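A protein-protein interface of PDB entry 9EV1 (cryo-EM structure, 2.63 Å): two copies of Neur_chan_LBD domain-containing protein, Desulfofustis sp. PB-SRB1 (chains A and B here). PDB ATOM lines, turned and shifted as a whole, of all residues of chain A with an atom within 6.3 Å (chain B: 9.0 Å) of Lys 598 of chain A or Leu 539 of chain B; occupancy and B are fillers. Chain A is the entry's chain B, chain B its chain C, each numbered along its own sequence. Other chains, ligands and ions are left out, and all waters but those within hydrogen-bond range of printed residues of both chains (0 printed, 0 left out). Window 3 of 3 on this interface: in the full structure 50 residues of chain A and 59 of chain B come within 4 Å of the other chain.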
ATOM      1  N   TYR A 542      22.005  -1.027   4.533  1.00  0.00           N
ATOM      2  CA  TYR A 542      22.425  -2.126   3.674  1.00  0.00           C
ATOM      3  C   TYR A 542      23.235  -1.666   2.468  1.00  0.00           C
ATOM      4  O   TYR A 542      23.943  -2.483   1.870  1.00  0.00           O
ATOM      5  CB  TYR A 542      21.200  -2.927   3.236  1.00  0.00           C
ATOM      6  CG  TYR A 542      20.430  -3.477   4.415  1.00  0.00           C
ATOM      7  CD1 TYR A 542      20.959  -4.491   5.201  1.00  0.00           C
ATOM      8  CD2 TYR A 542      19.183  -2.969   4.755  1.00  0.00           C
ATOM      9  CE1 TYR A 542      20.267  -4.991   6.286  1.00  0.00           C
ATOM     10  CE2 TYR A 542      18.484  -3.463   5.838  1.00  0.00           C
ATOM     11  CZ  TYR A 542      19.031  -4.474   6.600  1.00  0.00           C
ATOM     12  OH  TYR A 542      18.343  -4.971   7.681  1.00  0.00           O
ATOM     13  N   GLY A 543      23.167  -0.384   2.105  1.00  0.00           N
ATOM     14  CA  GLY A 543      24.043   0.115   1.058  1.00  0.00           C
ATOM     15  C   GLY A 543      25.506   0.054   1.455  1.00  0.00           C
ATOM     16  O   GLY A 543      26.356  -0.388   0.673  1.00  0.00           O
ATOM     17  N   LEU A 546      26.574  -3.614   1.410  1.00  0.00           N
ATOM     18  CA  LEU A 546      26.833  -4.089   0.056  1.00  0.00           C
ATOM     19  C   LEU A 546      28.153  -3.551  -0.479  1.00  0.00           C
ATOM     20  O   LEU A 546      28.934  -4.292  -1.090  1.00  0.00           O
ATOM     21  CB  LEU A 546      25.677  -3.695  -0.863  1.00  0.00           C
ATOM     22  CG  LEU A 546      25.815  -4.055  -2.342  1.00  0.00           C
ATOM     23  CD1 LEU A 546      26.111  -5.536  -2.505  1.00  0.00           C
ATOM     24  CD2 LEU A 546      24.557  -3.672  -3.104  1.00  0.00           C
ATOM     25  N   ILE A 593      23.712 -12.169  -0.648  1.00  0.00           N
ATOM     26  CA  ILE A 593      22.770 -11.941   0.444  1.00  0.00           C
ATOM     27  C   ILE A 593      22.626 -10.449   0.719  1.00  0.00           C
ATOM     28  O   ILE A 593      21.537  -9.969   1.059  1.00  0.00           O
ATOM     29  CB  ILE A 593      23.210 -12.714   1.702  1.00  0.00           C
ATOM     30  CG1 ILE A 593      23.210 -14.218   1.427  1.00  0.00           C
ATOM     31  CG2 ILE A 593      22.299 -12.396   2.875  1.00  0.00           C
ATOM     32  CD1 ILE A 593      23.682 -15.050   2.597  1.00  0.00           C
ATOM     33  N   SER A 594      23.718  -9.694   0.584  1.00  0.00           N
ATOM     34  CA  SER A 594      23.643  -8.249   0.775  1.00  0.00           C
ATOM     35  C   SER A 594      22.727  -7.604  -0.257  1.00  0.00           C
ATOM     36  O   SER A 594      21.935  -6.714   0.076  1.00  0.00           O
ATOM     37  CB  SER A 594      25.041  -7.636   0.708  1.00  0.00           C
ATOM     38  OG  SER A 594      25.879  -8.162   1.721  1.00  0.00           O
ATOM     39  N   VAL A 595      22.821  -8.036  -1.516  1.00  0.00           N
ATOM     40  CA  VAL A 595      21.926  -7.510  -2.548  1.00  0.00           C
ATOM     41  C   VAL A 595      20.476  -7.851  -2.219  1.00  0.00           C
ATOM     42  O   VAL A 595      19.573  -7.006  -2.346  1.00  0.00           O
ATOM     43  CB  VAL A 595      22.328  -8.045  -3.936  1.00  0.00           C
ATOM     44  CG1 VAL A 595      21.335  -7.584  -4.989  1.00  0.00           C
ATOM     45  CG2 VAL A 595      23.729  -7.592  -4.297  1.00  0.00           C
ATOM     46  N   CYS A 596      20.228  -9.094  -1.797  1.00  0.00           N
ATOM     47  CA  CYS A 596      18.865  -9.494  -1.452  1.00  0.00           C
ATOM     48  C   CYS A 596      18.313  -8.652  -0.306  1.00  0.00           C
ATOM     49  O   CYS A 596      17.155  -8.215  -0.343  1.00  0.00           O
ATOM     50  CB  CYS A 596      18.830 -10.979  -1.094  1.00  0.00           C
ATOM     51  SG  CYS A 596      17.195 -11.607  -0.646  1.00  0.00           S
ATOM     52  N   GLN A 597      19.131  -8.411   0.722  1.00  0.00           N
ATOM     53  CA  GLN A 597      18.693  -7.602   1.854  1.00  0.00           C
ATOM     54  C   GLN A 597      18.462  -6.153   1.447  1.00  0.00           C
ATOM     55  O   GLN A 597      17.541  -5.503   1.955  1.00  0.00           O
ATOM     56  CB  GLN A 597      19.715  -7.680   2.985  1.00  0.00           C
ATOM     57  CG  GLN A 597      19.707  -8.993   3.733  1.00  0.00           C
ATOM     58  CD  GLN A 597      20.662  -8.990   4.903  1.00  0.00           C
ATOM     59  OE1 GLN A 597      21.759  -8.439   4.823  1.00  0.00           O
ATOM     60  NE2 GLN A 597      20.244  -9.596   6.006  1.00  0.00           N
ATOM     61  N   LYS A 598      19.295  -5.622   0.552  1.00  0.00           N
ATOM     62  CA  LYS A 598      19.075  -4.268   0.059  1.00  0.00           C
ATOM     63  C   LYS A 598      17.728  -4.159  -0.643  1.00  0.00           C
ATOM     64  O   LYS A 598      16.975  -3.204  -0.416  1.00  0.00           O
ATOM     65  CB  LYS A 598      20.209  -3.859  -0.880  1.00  0.00           C
ATOM     66  CG  LYS A 598      20.017  -2.506  -1.543  1.00  0.00           C
ATOM     67  CD  LYS A 598      19.941  -1.393  -0.516  1.00  0.00           C
ATOM     68  CE  LYS A 598      19.822  -0.035  -1.186  1.00  0.00           C
ATOM     69  NZ  LYS A 598      18.618   0.047  -2.060  1.00  0.00           N
ATOM     70  N   ARG A 599      17.396  -5.143  -1.481  1.00  0.00           N
ATOM     71  CA  ARG A 599      16.090  -5.125  -2.138  1.00  0.00           C
ATOM     72  C   ARG A 599      14.954  -5.238  -1.125  1.00  0.00           C
ATOM     73  O   ARG A 599      13.953  -4.513  -1.219  1.00  0.00           O
ATOM     74  CB  ARG A 599      16.001  -6.248  -3.172  1.00  0.00           C
ATOM     75  CG  ARG A 599      14.691  -6.261  -3.944  1.00  0.00           C
ATOM     76  CD  ARG A 599      14.414  -4.905  -4.568  1.00  0.00           C
ATOM     77  NE  ARG A 599      13.058  -4.801  -5.093  1.00  0.00           N
ATOM     78  CZ  ARG A 599      12.515  -3.678  -5.542  1.00  0.00           C
ATOM     79  NH1 ARG A 599      13.187  -2.540  -5.545  1.00  0.00           N
ATOM     80  NH2 ARG A 599      11.264  -3.696  -5.991  1.00  0.00           N
ATOM     81  N   LEU A 600      15.091  -6.137  -0.146  1.00  0.00           N
ATOM     82  CA  LEU A 600      14.040  -6.304   0.856  1.00  0.00           C
ATOM     83  C   LEU A 600      13.823  -5.023   1.652  1.00  0.00           C
ATOM     84  O   LEU A 600      12.682  -4.659   1.958  1.00  0.00           O
ATOM     85  CB  LEU A 600      14.380  -7.463   1.793  1.00  0.00           C
ATOM     86  CG  LEU A 600      13.955  -8.861   1.345  1.00  0.00           C
ATOM     87  CD1 LEU A 600      14.340  -9.898   2.385  1.00  0.00           C
ATOM     88  CD2 LEU A 600      12.461  -8.894   1.085  1.00  0.00           C
ATOM     89  N   GLY A 601      14.906  -4.330   2.003  1.00  0.00           N
ATOM     90  CA  GLY A 601      14.765  -3.043   2.664  1.00  0.00           C
ATOM     91  C   GLY A 601      14.135  -1.998   1.765  1.00  0.00           C
ATOM     92  O   GLY A 601      13.379  -1.141   2.229  1.00  0.00           O
ATOM     93  N   ALA A 602      14.441  -2.051   0.466  1.00  0.00           N
ATOM     94  CA  ALA A 602      13.841  -1.109  -0.473  1.00  0.00           C
ATOM     95  C   ALA A 602      12.330  -1.295  -0.554  1.00  0.00           C
ATOM     96  O   ALA A 602      11.581  -0.315  -0.634  1.00  0.00           O
ATOM     97  CB  ALA A 602      14.475  -1.268  -1.854  1.00  0.00           C
ATOM     98  N   VAL A 603      11.861  -2.547  -0.534  1.00  0.00           N
ATOM     99  CA  VAL A 603      10.423  -2.805  -0.636  1.00  0.00           C
ATOM    100  C   VAL A 603       9.677  -2.531   0.661  1.00  0.00           C
ATOM    101  O   VAL A 603       8.454  -2.341   0.636  1.00  0.00           O
ATOM    102  CB  VAL A 603      10.189  -4.258  -1.098  1.00  0.00           C
ATOM    103  CG1 VAL A 603       8.719  -4.517  -1.390  1.00  0.00           C
ATOM    104  CG2 VAL A 603      11.016  -4.554  -2.337  1.00  0.00           C
ATOM    105  N   VAL B 532      26.552 -12.817  -9.467  1.00  0.00           N
ATOM    106  CA  VAL B 532      26.576 -11.497  -8.840  1.00  0.00           C
ATOM    107  C   VAL B 532      26.237 -10.421  -9.861  1.00  0.00           C
ATOM    108  O   VAL B 532      25.480  -9.486  -9.574  1.00  0.00           O
ATOM    109  CB  VAL B 532      27.941 -11.236  -8.175  1.00  0.00           C
ATOM    110  CG1 VAL B 532      28.034  -9.793  -7.706  1.00  0.00           C
ATOM    111  CG2 VAL B 532      28.153 -12.181  -7.006  1.00  0.00           C
ATOM    112  N   TRP B 534      24.393 -10.838 -12.491  1.00  0.00           N
ATOM    113  CA  TRP B 534      23.015 -11.010 -12.939  1.00  0.00           C
ATOM    114  C   TRP B 534      22.004 -10.543 -11.894  1.00  0.00           C
ATOM    115  O   TRP B 534      20.953  -9.996 -12.247  1.00  0.00           O
ATOM    116  CB  TRP B 534      22.774 -12.475 -13.299  1.00  0.00           C
ATOM    117  CG  TRP B 534      21.344 -12.818 -13.574  1.00  0.00           C
ATOM    118  CD1 TRP B 534      20.672 -12.651 -14.750  1.00  0.00           C
ATOM    119  CD2 TRP B 534      20.411 -13.402 -12.659  1.00  0.00           C
ATOM    120  NE1 TRP B 534      19.378 -13.086 -14.621  1.00  0.00           N
ATOM    121  CE2 TRP B 534      19.192 -13.553 -13.346  1.00  0.00           C
ATOM    122  CE3 TRP B 534      20.487 -13.806 -11.323  1.00  0.00           C
ATOM    123  CZ2 TRP B 534      18.061 -14.092 -12.746  1.00  0.00           C
ATOM    124  CZ3 TRP B 534      19.360 -14.341 -10.728  1.00  0.00           C
ATOM    125  CH2 TRP B 534      18.164 -14.479 -11.439  1.00  0.00           C
ATOM    126  N   VAL B 535      22.299 -10.750 -10.609  1.00  0.00           N
ATOM    127  CA  VAL B 535      21.306 -10.528  -9.563  1.00  0.00           C
ATOM    128  C   VAL B 535      21.009  -9.050  -9.333  1.00  0.00           C
ATOM    129  O   VAL B 535      19.959  -8.714  -8.772  1.00  0.00           O
ATOM    130  CB  VAL B 535      21.767 -11.198  -8.254  1.00  0.00           C
ATOM    131  CG1 VAL B 535      22.873 -10.388  -7.594  1.00  0.00           C
ATOM    132  CG2 VAL B 535      20.596 -11.404  -7.305  1.00  0.00           C
ATOM    133  N   ILE B 536      21.898  -8.149  -9.759  1.00  0.00           N
ATOM    134  CA  ILE B 536      21.753  -6.734  -9.433  1.00  0.00           C
ATOM    135  C   ILE B 536      20.613  -6.055 -10.176  1.00  0.00           C
ATOM    136  O   ILE B 536      20.266  -4.917  -9.844  1.00  0.00           O
ATOM    137  CB  ILE B 536      23.067  -5.979  -9.709  1.00  0.00           C
ATOM    138  CG1 ILE B 536      23.424  -6.046 -11.193  1.00  0.00           C
ATOM    139  CG2 ILE B 536      24.188  -6.556  -8.865  1.00  0.00           C
ATOM    140  CD1 ILE B 536      24.718  -5.345 -11.537  1.00  0.00           C
ATOM    141  N   PHE B 537      20.015  -6.717 -11.168  1.00  0.00           N
ATOM    142  CA  PHE B 537      18.938  -6.098 -11.931  1.00  0.00           C
ATOM    143  C   PHE B 537      17.602  -6.113 -11.199  1.00  0.00           C
ATOM    144  O   PHE B 537      16.630  -5.551 -11.715  1.00  0.00           O
ATOM    145  CB  PHE B 537      18.797  -6.779 -13.293  1.00  0.00           C
ATOM    146  CG  PHE B 537      19.809  -6.316 -14.304  1.00  0.00           C
ATOM    147  CD1 PHE B 537      21.050  -6.923 -14.394  1.00  0.00           C
ATOM    148  CD2 PHE B 537      19.520  -5.267 -15.159  1.00  0.00           C
ATOM    149  CE1 PHE B 537      21.981  -6.494 -15.320  1.00  0.00           C
ATOM    150  CE2 PHE B 537      20.446  -4.835 -16.087  1.00  0.00           C
ATOM    151  CZ  PHE B 537      21.677  -5.450 -16.166  1.00  0.00           C
ATOM    152  N   PHE B 538      17.523  -6.737 -10.022  1.00  0.00           N
ATOM    153  CA  PHE B 538      16.318  -6.631  -9.209  1.00  0.00           C
ATOM    154  C   PHE B 538      16.211  -5.283  -8.513  1.00  0.00           C
ATOM    155  O   PHE B 538      15.110  -4.890  -8.113  1.00  0.00           O
ATOM    156  CB  PHE B 538      16.273  -7.751  -8.168  1.00  0.00           C
ATOM    157  CG  PHE B 538      15.926  -9.095  -8.735  1.00  0.00           C
ATOM    158  CD1 PHE B 538      14.624  -9.394  -9.092  1.00  0.00           C
ATOM    159  CD2 PHE B 538      16.899 -10.067  -8.895  1.00  0.00           C
ATOM    160  CE1 PHE B 538      14.299 -10.632  -9.608  1.00  0.00           C
ATOM    161  CE2 PHE B 538      16.580 -11.307  -9.411  1.00  0.00           C
ATOM    162  CZ  PHE B 538      15.278 -11.590  -9.767  1.00  0.00           C
ATOM    163  N   LEU B 539      17.323  -4.573  -8.353  1.00  0.00           N
ATOM    164  CA  LEU B 539      17.309  -3.274  -7.699  1.00  0.00           C
ATOM    165  C   LEU B 539      16.624  -2.230  -8.576  1.00  0.00           C
ATOM    166  O   LEU B 539      16.681  -2.285  -9.807  1.00  0.00           O
ATOM    167  CB  LEU B 539      18.732  -2.822  -7.376  1.00  0.00           C
ATOM    168  CG  LEU B 539      19.541  -3.687  -6.408  1.00  0.00           C
ATOM    169  CD1 LEU B 539      20.957  -3.155  -6.280  1.00  0.00           C
ATOM    170  CD2 LEU B 539      18.866  -3.752  -5.047  1.00  0.00           C
ATOM    171  N   LYS B 540      15.967  -1.273  -7.923  1.00  0.00           N
ATOM    172  CA  LYS B 540      15.343  -0.150  -8.606  1.00  0.00           C
ATOM    173  C   LYS B 540      16.104   1.155  -8.410  1.00  0.00           C
ATOM    174  O   LYS B 540      15.689   2.186  -8.951  1.00  0.00           O
ATOM    175  CB  LYS B 540      13.891   0.012  -8.144  1.00  0.00           C
ATOM    176  CG  LYS B 540      12.967  -1.080  -8.655  1.00  0.00           C
ATOM    177  CD  LYS B 540      12.954  -1.109 -10.173  1.00  0.00           C
ATOM    178  CE  LYS B 540      12.145  -2.280 -10.707  1.00  0.00           C
ATOM    179  NZ  LYS B 540      12.749  -3.589 -10.336  1.00  0.00           N
ATOM    180  N   ASP B 541      17.200   1.140  -7.655  1.00  0.00           N
ATOM    181  CA  ASP B 541      18.102   2.283  -7.534  1.00  0.00           C
ATOM    182  C   ASP B 541      19.275   2.019  -8.470  1.00  0.00           C
ATOM    183  O   ASP B 541      20.148   1.200  -8.174  1.00  0.00           O
ATOM    184  CB  ASP B 541      18.556   2.469  -6.091  1.00  0.00           C
ATOM    185  CG  ASP B 541      19.357   3.741  -5.889  1.00  0.00           C
ATOM    186  OD1 ASP B 541      19.407   4.574  -6.819  1.00  0.00           O
ATOM    187  OD2 ASP B 541      19.940   3.906  -4.797  1.00  0.00           O
ATOM    188  N   TYR B 542      19.297   2.722  -9.604  1.00  0.00           N
ATOM    189  CA  TYR B 542      20.227   2.376 -10.672  1.00  0.00           C
ATOM    190  C   TYR B 542      21.650   2.849 -10.400  1.00  0.00           C
ATOM    191  O   TYR B 542      22.585   2.330 -11.019  1.00  0.00           O
ATOM    192  CB  TYR B 542      19.709   2.928 -12.000  1.00  0.00           C
ATOM    193  CG  TYR B 542      18.348   2.372 -12.352  1.00  0.00           C
ATOM    194  CD1 TYR B 542      18.201   1.048 -12.745  1.00  0.00           C
ATOM    195  CD2 TYR B 542      17.209   3.160 -12.270  1.00  0.00           C
ATOM    196  CE1 TYR B 542      16.962   0.528 -13.056  1.00  0.00           C
ATOM    197  CE2 TYR B 542      15.964   2.649 -12.582  1.00  0.00           C
ATOM    198  CZ  TYR B 542      15.847   1.332 -12.974  1.00  0.00           C
ATOM    199  OH  TYR B 542      14.612   0.812 -13.282  1.00  0.00           O
ATOM    200  N   GLY B 543      21.843   3.801  -9.487  1.00  0.00           N
ATOM    201  CA  GLY B 543      23.197   4.176  -9.111  1.00  0.00           C
ATOM    202  C   GLY B 543      23.932   3.051  -8.408  1.00  0.00           C
ATOM    203  O   GLY B 543      25.094   2.764  -8.717  1.00  0.00           O
ATOM    204  N   ARG B 544      23.260   2.389  -7.462  1.00  0.00           N
ATOM    205  CA  ARG B 544      23.849   1.230  -6.804  1.00  0.00           C
ATOM    206  C   ARG B 544      24.127   0.114  -7.802  1.00  0.00           C
ATOM    207  O   ARG B 544      25.171  -0.545  -7.735  1.00  0.00           O
ATOM    208  CB  ARG B 544      22.929   0.733  -5.689  1.00  0.00           C
ATOM    209  CG  ARG B 544      22.850   1.654  -4.484  1.00  0.00           C
ATOM    210  CD  ARG B 544      24.167   1.678  -3.726  1.00  0.00           C
ATOM    211  NE  ARG B 544      24.066   2.442  -2.488  1.00  0.00           N
ATOM    212  CZ  ARG B 544      25.054   2.589  -1.616  1.00  0.00           C
ATOM    213  NH1 ARG B 544      26.240   2.037  -1.817  1.00  0.00           N
ATOM    214  NH2 ARG B 544      24.849   3.306  -0.516  1.00  0.00           N
ATOM    215  N   GLN B 545      23.195  -0.118  -8.731  1.00  0.00           N
ATOM    216  CA  GLN B 545      23.398  -1.144  -9.748  1.00  0.00           C
ATOM    217  C   GLN B 545      24.620  -0.837 -10.605  1.00  0.00           C
ATOM    218  O   GLN B 545      25.443  -1.724 -10.868  1.00  0.00           O
ATOM    219  CB  GLN B 545      22.146  -1.267 -10.617  1.00  0.00           C
ATOM    220  CG  GLN B 545      22.309  -2.172 -11.825  1.00  0.00           C
ATOM    221  CD  GLN B 545      21.032  -2.304 -12.628  1.00  0.00           C
ATOM    222  OE1 GLN B 545      19.933  -2.275 -12.076  1.00  0.00           O
ATOM    223  NE2 GLN B 545      21.169  -2.444 -13.940  1.00  0.00           N
ATOM    224  N   LEU B 546      24.762   0.418 -11.039  1.00  0.00           N
ATOM    225  CA  LEU B 546      25.916   0.799 -11.846  1.00  0.00           C
ATOM    226  C   LEU B 546      27.215   0.636 -11.067  1.00  0.00           C
ATOM    227  O   LEU B 546      28.210   0.132 -11.603  1.00  0.00           O
ATOM    228  CB  LEU B 546      25.755   2.240 -12.332  1.00  0.00           C
ATOM    229  CG  LEU B 546      26.918   2.831 -13.130  1.00  0.00           C
ATOM    230  CD1 LEU B 546      27.257   1.946 -14.315  1.00  0.00           C
ATOM    231  CD2 LEU B 546      26.592   4.243 -13.586  1.00  0.00           C
ATOM    232  N   GLU B 547      27.226   1.056  -9.799  1.00  0.00           N
ATOM    233  CA  GLU B 547      28.435   0.930  -8.991  1.00  0.00           C
ATOM    234  C   GLU B 547      28.822  -0.531  -8.793  1.00  0.00           C
ATOM    235  O   GLU B 547      30.002  -0.893  -8.912  1.00  0.00           O
ATOM    236  CB  GLU B 547      28.235   1.623  -7.644  1.00  0.00           C
ATOM    237  CG  GLU B 547      29.485   1.682  -6.782  1.00  0.00           C
ATOM    238  CD  GLU B 547      29.279   2.482  -5.512  1.00  0.00           C
ATOM    239  OE1 GLU B 547      28.150   2.970  -5.292  1.00  0.00           O
ATOM    240  OE2 GLU B 547      30.245   2.625  -4.733  1.00  0.00           O
ATOM    241  N   VAL B 548      27.842  -1.390  -8.502  1.00  0.00           N
ATOM    242  CA  VAL B 548      28.139  -2.802  -8.285  1.00  0.00           C
ATOM    243  C   VAL B 548      28.609  -3.456  -9.578  1.00  0.00           C
ATOM    244  O   VAL B 548      29.504  -4.306  -9.563  1.00  0.00           O
ATOM    245  CB  VAL B 548      26.919  -3.524  -7.685  1.00  0.00           C
ATOM    246  CG1 VAL B 548      27.189  -5.014  -7.568  1.00  0.00           C
ATOM    247  CG2 VAL B 548      26.593  -2.953  -6.319  1.00  0.00           C
ATOM    248  N   ALA B 549      28.026  -3.073 -10.718  1.00  0.00           N
ATOM    249  CA  ALA B 549      28.493  -3.607 -11.995  1.00  0.00           C
ATOM    250  C   ALA B 549      29.930  -3.187 -12.280  1.00  0.00           C
ATOM    251  O   ALA B 549      30.749  -3.999 -12.737  1.00  0.00           O
ATOM    252  CB  ALA B 549      27.567  -3.154 -13.122  1.00  0.00           C
ATOM    253  N   GLN B 597      20.221   2.649 -18.407  1.00  0.00           N
ATOM    254  CA  GLN B 597      19.081   2.691 -17.497  1.00  0.00           C
ATOM    255  C   GLN B 597      19.170   3.877 -16.547  1.00  0.00           C
ATOM    256  O   GLN B 597      18.149   4.485 -16.211  1.00  0.00           O
ATOM    257  CB  GLN B 597      18.988   1.387 -16.709  1.00  0.00           C
ATOM    258  CG  GLN B 597      18.541   0.201 -17.532  1.00  0.00           C
ATOM    259  CD  GLN B 597      18.409  -1.054 -16.705  1.00  0.00           C
ATOM    260  OE1 GLN B 597      19.279  -1.375 -15.897  1.00  0.00           O
ATOM    261  NE2 GLN B 597      17.310  -1.771 -16.894  1.00  0.00           N
ATOM    262  N   ALA B 609      12.858   1.476 -18.010  1.00  0.00           N
ATOM    263  CA  ALA B 609      13.969   0.868 -17.287  1.00  0.00           C
ATOM    264  C   ALA B 609      13.554  -0.442 -16.627  1.00  0.00           C
ATOM    265  O   ALA B 609      14.307  -1.424 -16.650  1.00  0.00           O
ATOM    266  CB  ALA B 609      14.515   1.848 -16.252  1.00  0.00           C
ATOM    267  N   ALA B 610      12.359  -0.479 -16.032  1.00  0.00           N
ATOM    268  CA  ALA B 610      11.871  -1.721 -15.439  1.00  0.00           C
ATOM    269  C   ALA B 610      11.675  -2.799 -16.499  1.00  0.00           C
ATOM    270  O   ALA B 610      11.995  -3.976 -16.274  1.00  0.00           O
ATOM    271  CB  ALA B 610      10.569  -1.464 -14.682  1.00  0.00           C
ATOM    272  N   ASP B 613      14.987  -4.160 -17.356  1.00  0.00           N
ATOM    273  CA  ASP B 613      15.435  -5.048 -16.287  1.00  0.00           C
ATOM    274  C   ASP B 613      14.831  -6.437 -16.443  1.00  0.00           C
ATOM    275  O   ASP B 613      15.537  -7.451 -16.359  1.00  0.00           O
ATOM    276  CB  ASP B 613      15.070  -4.458 -14.924  1.00  0.00           C
ATOM    277  CG  ASP B 613      15.911  -3.251 -14.563  1.00  0.00           C
ATOM    278  OD1 ASP B 613      17.086  -3.199 -14.983  1.00  0.00           O
ATOM    279  OD2 ASP B 613      15.402  -2.357 -13.855  1.00  0.00           O
ATOM    280  N   THR B 614      13.517  -6.498 -16.678  1.00  0.00           N
ATOM    281  CA  THR B 614      12.865  -7.792 -16.867  1.00  0.00           C
ATOM    282  C   THR B 614      13.431  -8.523 -18.079  1.00  0.00           C
ATOM    283  O   THR B 614      13.697  -9.733 -18.020  1.00  0.00           O
ATOM    284  CB  THR B 614      11.354  -7.608 -17.014  1.00  0.00           C
ATOM    285  OG1 THR B 614      11.081  -6.740 -18.120  1.00  0.00           O
ATOM    286  CG2 THR B 614      10.762  -7.011 -15.747  1.00  0.00           C
ATOM    287  N   LEU B 617      16.924  -9.900 -17.252  1.00  0.00           N
ATOM    288  CA  LEU B 617      16.807 -11.017 -16.319  1.00  0.00           C
ATOM    289  C   LEU B 617      16.342 -12.282 -17.024  1.00  0.00           C
ATOM    290  O   LEU B 617      16.790 -13.386 -16.696  1.00  0.00           O
ATOM    291  CB  LEU B 617      15.846 -10.661 -15.185  1.00  0.00           C
ATOM    292  CG  LEU B 617      16.334  -9.711 -14.092  1.00  0.00           C
ATOM    293  CD1 LEU B 617      15.181  -9.308 -13.191  1.00  0.00           C
ATOM    294  CD2 LEU B 617      17.443 -10.357 -13.282  1.00  0.00           C
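O of Gly 543 of chain A lies within hydrogen-bond range of NH1 of Arg 544 of chain B, at 3.5 Å.
The backbone carbonyl oxygen (O) of Phe 538 of chain B lies within hydrogen-bond range of the side-chain amino group (NZ) of Lys 540 of chain B.
CG2 of Val 548 of chain B touches CD2 of Leu 546 of chain A, 3.9 Å away. Leu 539 of chain B touches Lys 598 of chain A. O of Phe 538 of chain B touches CD of Arg 599 of chain A, at 3.6 Å. Lys 540 of chain B touches Arg 599 of chain A.
Printed residues of chain B within 4 Å of Leu 546 of chain A: Val 548. Of chain B, only Leu 539 comes within 4 Å of Lys 598 of chain A. Of the printed residues of chain B, Arg 599 of chain A touches Phe 538 (3.6 Å) and Lys 540 (3.4 Å). No residue of chain B comes within 4 Å of Gly 601 of chain A. Leu 539 of chain B touches just one residue of chain A: Lys 598 (3.9 Å). Of the printed residues of chain A, Arg 544 of chain B touches Gly 543 (3.5 Å). Printed residues of chain A within 4 Å of Val 548 of chain B: Leu 546.
Printed residues of chain A that touch a printed residue of chain B: Gly 543, Leu 546, Lys 598 and Arg 599. Hydrophobic or aromatic side chains of chain A within 4 Å of the printed part of chain B: Leu 546. Along chain B the printed residues that touch a printed residue of chain A span positions 538 to 548.
4 positions are printed for both chains.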
